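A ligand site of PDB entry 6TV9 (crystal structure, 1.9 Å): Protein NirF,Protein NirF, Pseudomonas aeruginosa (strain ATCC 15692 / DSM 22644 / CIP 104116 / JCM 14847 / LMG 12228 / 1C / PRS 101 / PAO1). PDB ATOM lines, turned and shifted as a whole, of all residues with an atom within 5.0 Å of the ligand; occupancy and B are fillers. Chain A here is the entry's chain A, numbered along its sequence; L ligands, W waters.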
ATOM      1  N   ARG A  21      -0.461   9.593 -27.469  1.00  0.00           N
ATOM      2  CA  ARG A  21       0.977   9.798 -27.560  1.00  0.00           C
ATOM      3  C   ARG A  21       1.550   9.405 -28.921  1.00  0.00           C
ATOM      4  O   ARG A  21       2.503  10.035 -29.391  1.00  0.00           O
ATOM      5  CB  ARG A  21       1.669   8.973 -26.450  1.00  0.00           C
ATOM      6  CG  ARG A  21       3.067   9.439 -26.090  1.00  0.00           C
ATOM      7  CD  ARG A  21       3.765   8.393 -25.249  1.00  0.00           C
ATOM      8  NE  ARG A  21       4.919   8.923 -24.540  1.00  0.00           N
ATOM      9  CZ  ARG A  21       6.151   8.993 -25.061  1.00  0.00           C
ATOM     10  NH1 ARG A  21       6.402   8.565 -26.302  1.00  0.00           N
ATOM     11  NH2 ARG A  21       7.149   9.501 -24.328  1.00  0.00           N
ATOM     12  N   HIS A  48       6.046  13.739 -26.539  1.00  0.00           N
ATOM     13  CA  HIS A  48       6.119  14.456 -25.259  1.00  0.00           C
ATOM     14  C   HIS A  48       5.420  15.782 -25.446  1.00  0.00           C
ATOM     15  O   HIS A  48       5.776  16.558 -26.327  1.00  0.00           O
ATOM     16  CB  HIS A  48       7.569  14.659 -24.818  1.00  0.00           C
ATOM     17  CG  HIS A  48       7.812  14.326 -23.392  1.00  0.00           C
ATOM     18  ND1 HIS A  48       7.621  13.055 -22.893  1.00  0.00           N
ATOM     19  CD2 HIS A  48       8.197  15.087 -22.351  1.00  0.00           C
ATOM     20  CE1 HIS A  48       7.892  13.048 -21.601  1.00  0.00           C
ATOM     21  NE2 HIS A  48       8.237  14.274 -21.248  1.00  0.00           N
ATOM     22  N   ALA A  49       4.399  16.053 -24.611  1.00  0.00           N
ATOM     23  CA  ALA A  49       3.579  17.231 -24.825  1.00  0.00           C
ATOM     24  C   ALA A  49       3.099  17.793 -23.501  1.00  0.00           C
ATOM     25  O   ALA A  49       2.952  17.092 -22.513  1.00  0.00           O
ATOM     26  CB  ALA A  49       2.363  16.907 -25.700  1.00  0.00           C
ATOM     27  N   SER A  50       2.841  19.108 -23.518  1.00  0.00           N
ATOM     28  CA  SER A  50       2.275  19.827 -22.383  1.00  0.00           C
ATOM     29  C   SER A  50       1.245  20.805 -22.929  1.00  0.00           C
ATOM     30  O   SER A  50       1.188  21.072 -24.130  1.00  0.00           O
ATOM     31  CB  SER A  50       3.344  20.541 -21.551  1.00  0.00           C
ATOM     32  OG  SER A  50       3.563  21.845 -22.040  1.00  0.00           O
ATOM     33  N   ARG A  65       6.731  18.109 -28.956  1.00  0.00           N
ATOM     34  CA  ARG A  65       8.169  17.982 -29.069  1.00  0.00           C
ATOM     35  C   ARG A  65       8.686  18.304 -30.468  1.00  0.00           C
ATOM     36  O   ARG A  65       9.891  18.443 -30.649  1.00  0.00           O
ATOM     37  CB  ARG A  65       8.605  16.564 -28.671  1.00  0.00           C
ATOM     38  CG  ARG A  65      10.114  16.457 -28.390  1.00  0.00           C
ATOM     39  CD  ARG A  65      10.635  15.046 -28.675  1.00  0.00           C
ATOM     40  NE  ARG A  65      10.599  14.190 -27.494  1.00  0.00           N
ATOM     41  CZ  ARG A  65      10.407  12.877 -27.521  1.00  0.00           C
ATOM     42  NH1 ARG A  65      10.219  12.250 -28.680  1.00  0.00           N
ATOM     43  NH2 ARG A  65      10.404  12.179 -26.386  1.00  0.00           N
ATOM     44  N   ILE A  90       8.761  22.009 -24.889  1.00  0.00           N
ATOM     45  CA  ILE A  90       7.419  21.973 -24.300  1.00  0.00           C
ATOM     46  C   ILE A  90       7.472  22.650 -22.937  1.00  0.00           C
ATOM     47  O   ILE A  90       8.503  23.194 -22.525  1.00  0.00           O
ATOM     48  CB  ILE A  90       6.900  20.532 -24.205  1.00  0.00           C
ATOM     49  CG1 ILE A  90       7.665  19.719 -23.181  1.00  0.00           C
ATOM     50  CG2 ILE A  90       6.986  19.848 -25.553  1.00  0.00           C
ATOM     51  CD1 ILE A  90       7.056  18.339 -22.930  1.00  0.00           C
ATOM     52  N   GLY A  91       6.347  22.637 -22.215  1.00  0.00           N
ATOM     53  CA  GLY A  91       6.289  23.294 -20.923  1.00  0.00           C
ATOM     54  C   GLY A  91       6.052  24.785 -20.968  1.00  0.00           C
ATOM     55  O   GLY A  91       6.478  25.506 -20.073  1.00  0.00           O
ATOM     56  N   TYR A 234      18.607  13.513 -17.777  1.00  0.00           N
ATOM     57  CA  TYR A 234      17.240  13.095 -18.028  1.00  0.00           C
ATOM     58  C   TYR A 234      16.719  12.108 -16.994  1.00  0.00           C
ATOM     59  O   TYR A 234      15.570  11.672 -17.103  1.00  0.00           O
ATOM     60  CB  TYR A 234      17.109  12.486 -19.428  1.00  0.00           C
ATOM     61  CG  TYR A 234      18.081  11.383 -19.738  1.00  0.00           C
ATOM     62  CD1 TYR A 234      17.870  10.094 -19.281  1.00  0.00           C
ATOM     63  CD2 TYR A 234      19.190  11.618 -20.529  1.00  0.00           C
ATOM     64  CE1 TYR A 234      18.757   9.079 -19.572  1.00  0.00           C
ATOM     65  CE2 TYR A 234      20.098  10.610 -20.824  1.00  0.00           C
ATOM     66  CZ  TYR A 234      19.868   9.348 -20.341  1.00  0.00           C
ATOM     67  OH  TYR A 234      20.752   8.338 -20.640  1.00  0.00           O
ATOM     68  N   LYS A 235      17.519  11.757 -15.988  1.00  0.00           N
ATOM     69  CA  LYS A 235      17.041  10.993 -14.844  1.00  0.00           C
ATOM     70  C   LYS A 235      16.846  11.862 -13.618  1.00  0.00           C
ATOM     71  O   LYS A 235      16.677  11.340 -12.512  1.00  0.00           O
ATOM     72  CB  LYS A 235      17.990   9.833 -14.544  1.00  0.00           C
ATOM     73  CG  LYS A 235      17.866   8.673 -15.531  1.00  0.00           C
ATOM     74  CD  LYS A 235      18.113   7.334 -14.885  1.00  0.00           C
ATOM     75  CE  LYS A 235      17.928   6.191 -15.888  1.00  0.00           C
ATOM     76  NZ  LYS A 235      16.517   6.100 -16.382  1.00  0.00           N
ATOM     77  N   HIS A 238      11.042  15.280 -12.661  1.00  0.00           N
ATOM     78  CA  HIS A 238      10.114  16.291 -13.110  1.00  0.00           C
ATOM     79  C   HIS A 238       9.735  17.157 -11.901  1.00  0.00           C
ATOM     80  O   HIS A 238       9.173  16.634 -10.929  1.00  0.00           O
ATOM     81  CB  HIS A 238       8.854  15.669 -13.699  1.00  0.00           C
ATOM     82  CG  HIS A 238       9.042  15.089 -15.056  1.00  0.00           C
ATOM     83  ND1 HIS A 238       9.947  14.084 -15.334  1.00  0.00           N
ATOM     84  CD2 HIS A 238       8.412  15.362 -16.235  1.00  0.00           C
ATOM     85  CE1 HIS A 238       9.868  13.774 -16.616  1.00  0.00           C
ATOM     86  NE2 HIS A 238       8.946  14.526 -17.181  1.00  0.00           N
ATOM     87  N   GLU A 240       7.467  19.415 -12.022  1.00  0.00           N
ATOM     88  CA  GLU A 240       6.015  19.352 -12.008  1.00  0.00           C
ATOM     89  C   GLU A 240       5.536  18.139 -11.210  1.00  0.00           C
ATOM     90  O   GLU A 240       4.373  18.090 -10.831  1.00  0.00           O
ATOM     91  CB  GLU A 240       5.454  19.292 -13.419  1.00  0.00           C
ATOM     92  CG  GLU A 240       5.288  20.665 -14.086  1.00  0.00           C
ATOM     93  CD  GLU A 240       4.234  21.535 -13.391  1.00  0.00           C
ATOM     94  OE1 GLU A 240       4.551  22.181 -12.362  1.00  0.00           O
ATOM     95  OE2 GLU A 240       3.072  21.554 -13.887  1.00  0.00           O
ATOM     96  N   VAL A 280       7.755   9.363 -10.160  1.00  0.00           N
ATOM     97  CA  VAL A 280       7.835  10.423 -11.156  1.00  0.00           C
ATOM     98  C   VAL A 280       7.014  11.624 -10.726  1.00  0.00           C
ATOM     99  O   VAL A 280       7.558  12.695 -10.445  1.00  0.00           O
ATOM    100  CB  VAL A 280       7.405   9.907 -12.549  1.00  0.00           C
ATOM    101  CG1 VAL A 280       7.566  11.002 -13.592  1.00  0.00           C
ATOM    102  CG2 VAL A 280       8.227   8.688 -12.928  1.00  0.00           C
ATOM    103  N   PHE A 281       5.686  11.459 -10.641  1.00  0.00           N
ATOM    104  CA  PHE A 281       4.788  12.522 -10.236  1.00  0.00           C
ATOM    105  C   PHE A 281       4.248  12.221  -8.864  1.00  0.00           C
ATOM    106  O   PHE A 281       3.662  11.157  -8.637  1.00  0.00           O
ATOM    107  CB  PHE A 281       3.651  12.691 -11.253  1.00  0.00           C
ATOM    108  CG  PHE A 281       4.103  13.098 -12.618  1.00  0.00           C
ATOM    109  CD1 PHE A 281       4.449  14.388 -12.874  1.00  0.00           C
ATOM    110  CD2 PHE A 281       4.182  12.173 -13.630  1.00  0.00           C
ATOM    111  CE1 PHE A 281       4.877  14.773 -14.142  1.00  0.00           C
ATOM    112  CE2 PHE A 281       4.610  12.544 -14.894  1.00  0.00           C
ATOM    113  CZ  PHE A 281       4.953  13.851 -15.138  1.00  0.00           C
ATOM    114  N   LEU A 324       1.034   6.759 -16.972  1.00  0.00           N
ATOM    115  CA  LEU A 324       1.918   7.891 -17.236  1.00  0.00           C
ATOM    116  C   LEU A 324       1.555   9.159 -16.462  1.00  0.00           C
ATOM    117  O   LEU A 324       2.462   9.862 -16.006  1.00  0.00           O
ATOM    118  CB  LEU A 324       1.919   8.217 -18.728  1.00  0.00           C
ATOM    119  CG  LEU A 324       2.660   7.260 -19.661  1.00  0.00           C
ATOM    120  CD1 LEU A 324       2.572   7.732 -21.106  1.00  0.00           C
ATOM    121  CD2 LEU A 324       4.113   7.127 -19.235  1.00  0.00           C
ATOM    122  N   HIS A 325       0.264   9.472 -16.320  1.00  0.00           N
ATOM    123  CA  HIS A 325      -0.117  10.770 -15.760  1.00  0.00           C
ATOM    124  C   HIS A 325      -1.416  10.620 -15.011  1.00  0.00           C
ATOM    125  O   HIS A 325      -2.197   9.701 -15.257  1.00  0.00           O
ATOM    126  CB  HIS A 325      -0.256  11.824 -16.875  1.00  0.00           C
ATOM    127  CG  HIS A 325      -0.226  13.232 -16.370  1.00  0.00           C
ATOM    128  ND1 HIS A 325      -1.173  14.161 -16.703  1.00  0.00           N
ATOM    129  CD2 HIS A 325       0.662  13.877 -15.563  1.00  0.00           C
ATOM    130  CE1 HIS A 325      -0.883  15.327 -16.125  1.00  0.00           C
ATOM    131  NE2 HIS A 325       0.238  15.177 -15.433  1.00  0.00           N
ATOM    132  N   ARG A 340      -1.311   3.912 -20.611  1.00  0.00           N
ATOM    133  CA  ARG A 340      -0.874   3.971 -22.003  1.00  0.00           C
ATOM    134  C   ARG A 340      -1.037   2.619 -22.684  1.00  0.00           C
ATOM    135  O   ARG A 340      -1.765   2.489 -23.677  1.00  0.00           O
ATOM    136  CB  ARG A 340       0.575   4.440 -22.084  1.00  0.00           C
ATOM    137  CG  ARG A 340       1.122   4.526 -23.503  1.00  0.00           C
ATOM    138  CD  ARG A 340       2.609   4.806 -23.523  1.00  0.00           C
ATOM    139  NE  ARG A 340       3.351   3.873 -22.675  1.00  0.00           N
ATOM    140  CZ  ARG A 340       4.648   3.935 -22.448  1.00  0.00           C
ATOM    141  NH1 ARG A 340       5.381   4.891 -23.014  1.00  0.00           N
ATOM    142  NH2 ARG A 340       5.220   3.043 -21.642  1.00  0.00           N
ATOM    143  N   GLY A 366      -0.605  12.381 -21.264  1.00  0.00           N
ATOM    144  CA  GLY A 366      -1.007  13.500 -20.435  1.00  0.00           C
ATOM    145  C   GLY A 366      -2.509  13.735 -20.478  1.00  0.00           C
ATOM    146  O   GLY A 366      -3.132  13.720 -21.525  1.00  0.00           O
ATOM    147  N   PHE A 368      -5.228  16.607 -18.956  1.00  0.00           N
ATOM    148  CA  PHE A 368      -5.300  17.937 -18.400  1.00  0.00           C
ATOM    149  C   PHE A 368      -6.736  18.428 -18.409  1.00  0.00           C
ATOM    150  O   PHE A 368      -7.468  18.175 -19.370  1.00  0.00           O
ATOM    151  CB  PHE A 368      -4.439  18.930 -19.172  1.00  0.00           C
ATOM    152  CG  PHE A 368      -3.071  18.400 -19.546  1.00  0.00           C
ATOM    153  CD1 PHE A 368      -2.926  17.476 -20.558  1.00  0.00           C
ATOM    154  CD2 PHE A 368      -1.939  18.866 -18.923  1.00  0.00           C
ATOM    155  CE1 PHE A 368      -1.690  17.016 -20.919  1.00  0.00           C
ATOM    156  CE2 PHE A 368      -0.691  18.400 -19.280  1.00  0.00           C
ATOM    157  CZ  PHE A 368      -0.576  17.484 -20.287  1.00  0.00           C
HETATM  158 FE1  LIG L   1       8.549  14.374 -19.208  1.00  0.00          FE
HETATM  159  C1  LIG L   1       5.816  16.548 -19.056  1.00  0.00           C
HETATM  160  C2  LIG L   1      10.849  17.064 -19.549  1.00  0.00           C
HETATM  161  C3  LIG L   1      11.236  12.126 -19.713  1.00  0.00           C
HETATM  162  C4  LIG L   1       6.438  11.694 -18.478  1.00  0.00           C
HETATM  163  N1  LIG L   1       8.390  16.365 -19.302  1.00  0.00           N
HETATM  164  C5  LIG L   1       7.162  17.125 -19.187  1.00  0.00           C
HETATM  165  C6  LIG L   1       7.403  18.585 -19.219  1.00  0.00           C
HETATM  166  C7  LIG L   1       8.873  18.746 -19.378  1.00  0.00           C
HETATM  167  C8  LIG L   1       9.426  17.358 -19.404  1.00  0.00           C
HETATM  168  C9  LIG L   1       9.639  20.031 -19.464  1.00  0.00           C
HETATM  169  C10 LIG L   1       6.351  19.671 -19.131  1.00  0.00           C
HETATM  170  C11 LIG L   1       6.098  20.034 -17.666  1.00  0.00           C
HETATM  171  C12 LIG L   1       5.304  21.308 -17.619  1.00  0.00           C
HETATM  172  O1  LIG L   1       5.929  22.404 -17.623  1.00  0.00           O
HETATM  173  O2  LIG L   1       4.058  21.228 -17.585  1.00  0.00           O
HETATM  174  N2  LIG L   1      10.639  14.572 -19.558  1.00  0.00           N
HETATM  175  C13 LIG L   1      11.365  15.699 -19.659  1.00  0.00           C
HETATM  176  C14 LIG L   1      12.754  15.334 -19.915  1.00  0.00           C
HETATM  177  O3  LIG L   1      13.691  16.209 -20.045  1.00  0.00           O
HETATM  178  C15 LIG L   1      12.989  13.903 -19.955  1.00  0.00           C
HETATM  179  C16 LIG L   1      13.822  13.525 -18.726  1.00  0.00           C
HETATM  180  C17 LIG L   1      13.604  13.430 -21.261  1.00  0.00           C
HETATM  181  C18 LIG L   1      12.546  13.189 -22.311  1.00  0.00           C
HETATM  182  O4  LIG L   1      12.037  14.188 -22.876  1.00  0.00           O
HETATM  183  O5  LIG L   1      12.202  12.008 -22.595  1.00  0.00           O
HETATM  184  C19 LIG L   1      11.550  13.565 -19.751  1.00  0.00           C
HETATM  185  N3  LIG L   1       8.779  12.313 -19.115  1.00  0.00           N
HETATM  186  C20 LIG L   1       9.918  11.592 -19.334  1.00  0.00           C
HETATM  187  C21 LIG L   1       9.606  10.179 -19.151  1.00  0.00           C
HETATM  188  O6  LIG L   1      10.493   9.257 -19.289  1.00  0.00           O
HETATM  189  C22 LIG L   1       8.228   9.916 -18.753  1.00  0.00           C
HETATM  190  C23 LIG L   1       8.248   9.468 -17.290  1.00  0.00           C
HETATM  191  C24 LIG L   1       7.453   8.913 -19.622  1.00  0.00           C
HETATM  192  C25 LIG L   1       7.455   9.210 -21.083  1.00  0.00           C
HETATM  193  O7  LIG L   1       6.658   8.563 -21.789  1.00  0.00           O
HETATM  194  O8  LIG L   1       8.215  10.094 -21.556  1.00  0.00           O
HETATM  195  C26 LIG L   1       7.829  11.370 -18.809  1.00  0.00           C
HETATM  196  N4  LIG L   1       6.492  14.177 -18.834  1.00  0.00           N
HETATM  197  C27 LIG L   1       5.820  13.032 -18.562  1.00  0.00           C
HETATM  198  C28 LIG L   1       4.366  13.190 -18.345  1.00  0.00           C
HETATM  199  C29 LIG L   1       4.146  14.624 -18.513  1.00  0.00           C
HETATM  200  C30 LIG L   1       5.526  15.123 -18.800  1.00  0.00           C
HETATM  201  C31 LIG L   1       3.338  12.147 -18.050  1.00  0.00           C
HETATM  202  C32 LIG L   1       2.786  15.285 -18.335  1.00  0.00           C
HETATM  203  C33 LIG L   1       2.624  16.716 -18.810  1.00  0.00           C
HETATM  204  C34 LIG L   1       2.931  17.734 -17.739  1.00  0.00           C
HETATM  205  O9  LIG L   1       3.297  18.886 -18.124  1.00  0.00           O
HETATM  206  O10 LIG L   1       2.832  17.433 -16.536  1.00  0.00           O
HETATM  207  O   HOH W   1       1.589  19.684 -15.137  1.00  0.00           O
HETATM  208  O   HOH W   2       6.021  24.503 -15.161  1.00  0.00           O
HETATM  209  O   HOH W   3      14.176  19.284 -20.005  1.00  0.00           O
HETATM  210  O   HOH W   4       9.570  10.063 -24.372  1.00  0.00           O
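FE1 of the ligand is bound by NE2 of His 48, at 2.1 Å. An iron atom (FE1) of the ligand is bound by a ring nitrogen (NE2) of His 238 (2.1 Å). The guanidinium group (NH2) of Arg 21 lies within salt-bridge range of an oxygen (O7) of the ligand.
Ala 49 touches the ligand (O to C33, 3.7 Å). Ser 50 touches the ligand. CD1 of Ile 90 touches C6 of the ligand, 3.7 Å away. CA of Gly 91 touches O1 of the ligand, 3.4 Å away. O of Tyr 234 touches C16 of the ligand, 3.0 Å away. CG of Glu 240 touches C12 of the ligand, 3.6 Å away. Phe 281 touches the ligand. Leu 324 touches the ligand (O to C31, 3.2 Å). His 325 touches the ligand (NE2 to O10, 3.6 Å). Phe 368 touches the ligand. Within 4 Å of the ligand: Arg 21, His 48, Ala 49, Ser 50, Ile 90, Gly 91, Tyr 234, His 238, Glu 240, Phe 281, Leu 324, His 325 and Phe 368.
Water W1 bridges OE2 of Glu 240 and O10 of the ligand. Water W4 lies within hydrogen-bond range of the guanidinium group of Arg 21, the guanidinium group of Arg 65 and an oxygen (O8) of the ligand.
The backbone carbonyl oxygen (O) of His 48 lies within hydrogen-bond range of the backbone NH (N) of Arg 65 (3.2 Å). The backbone NH of Gly 91 is in hydrogen-bond range of the side-chain hydroxyl of Ser 50 (2.9 Å).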
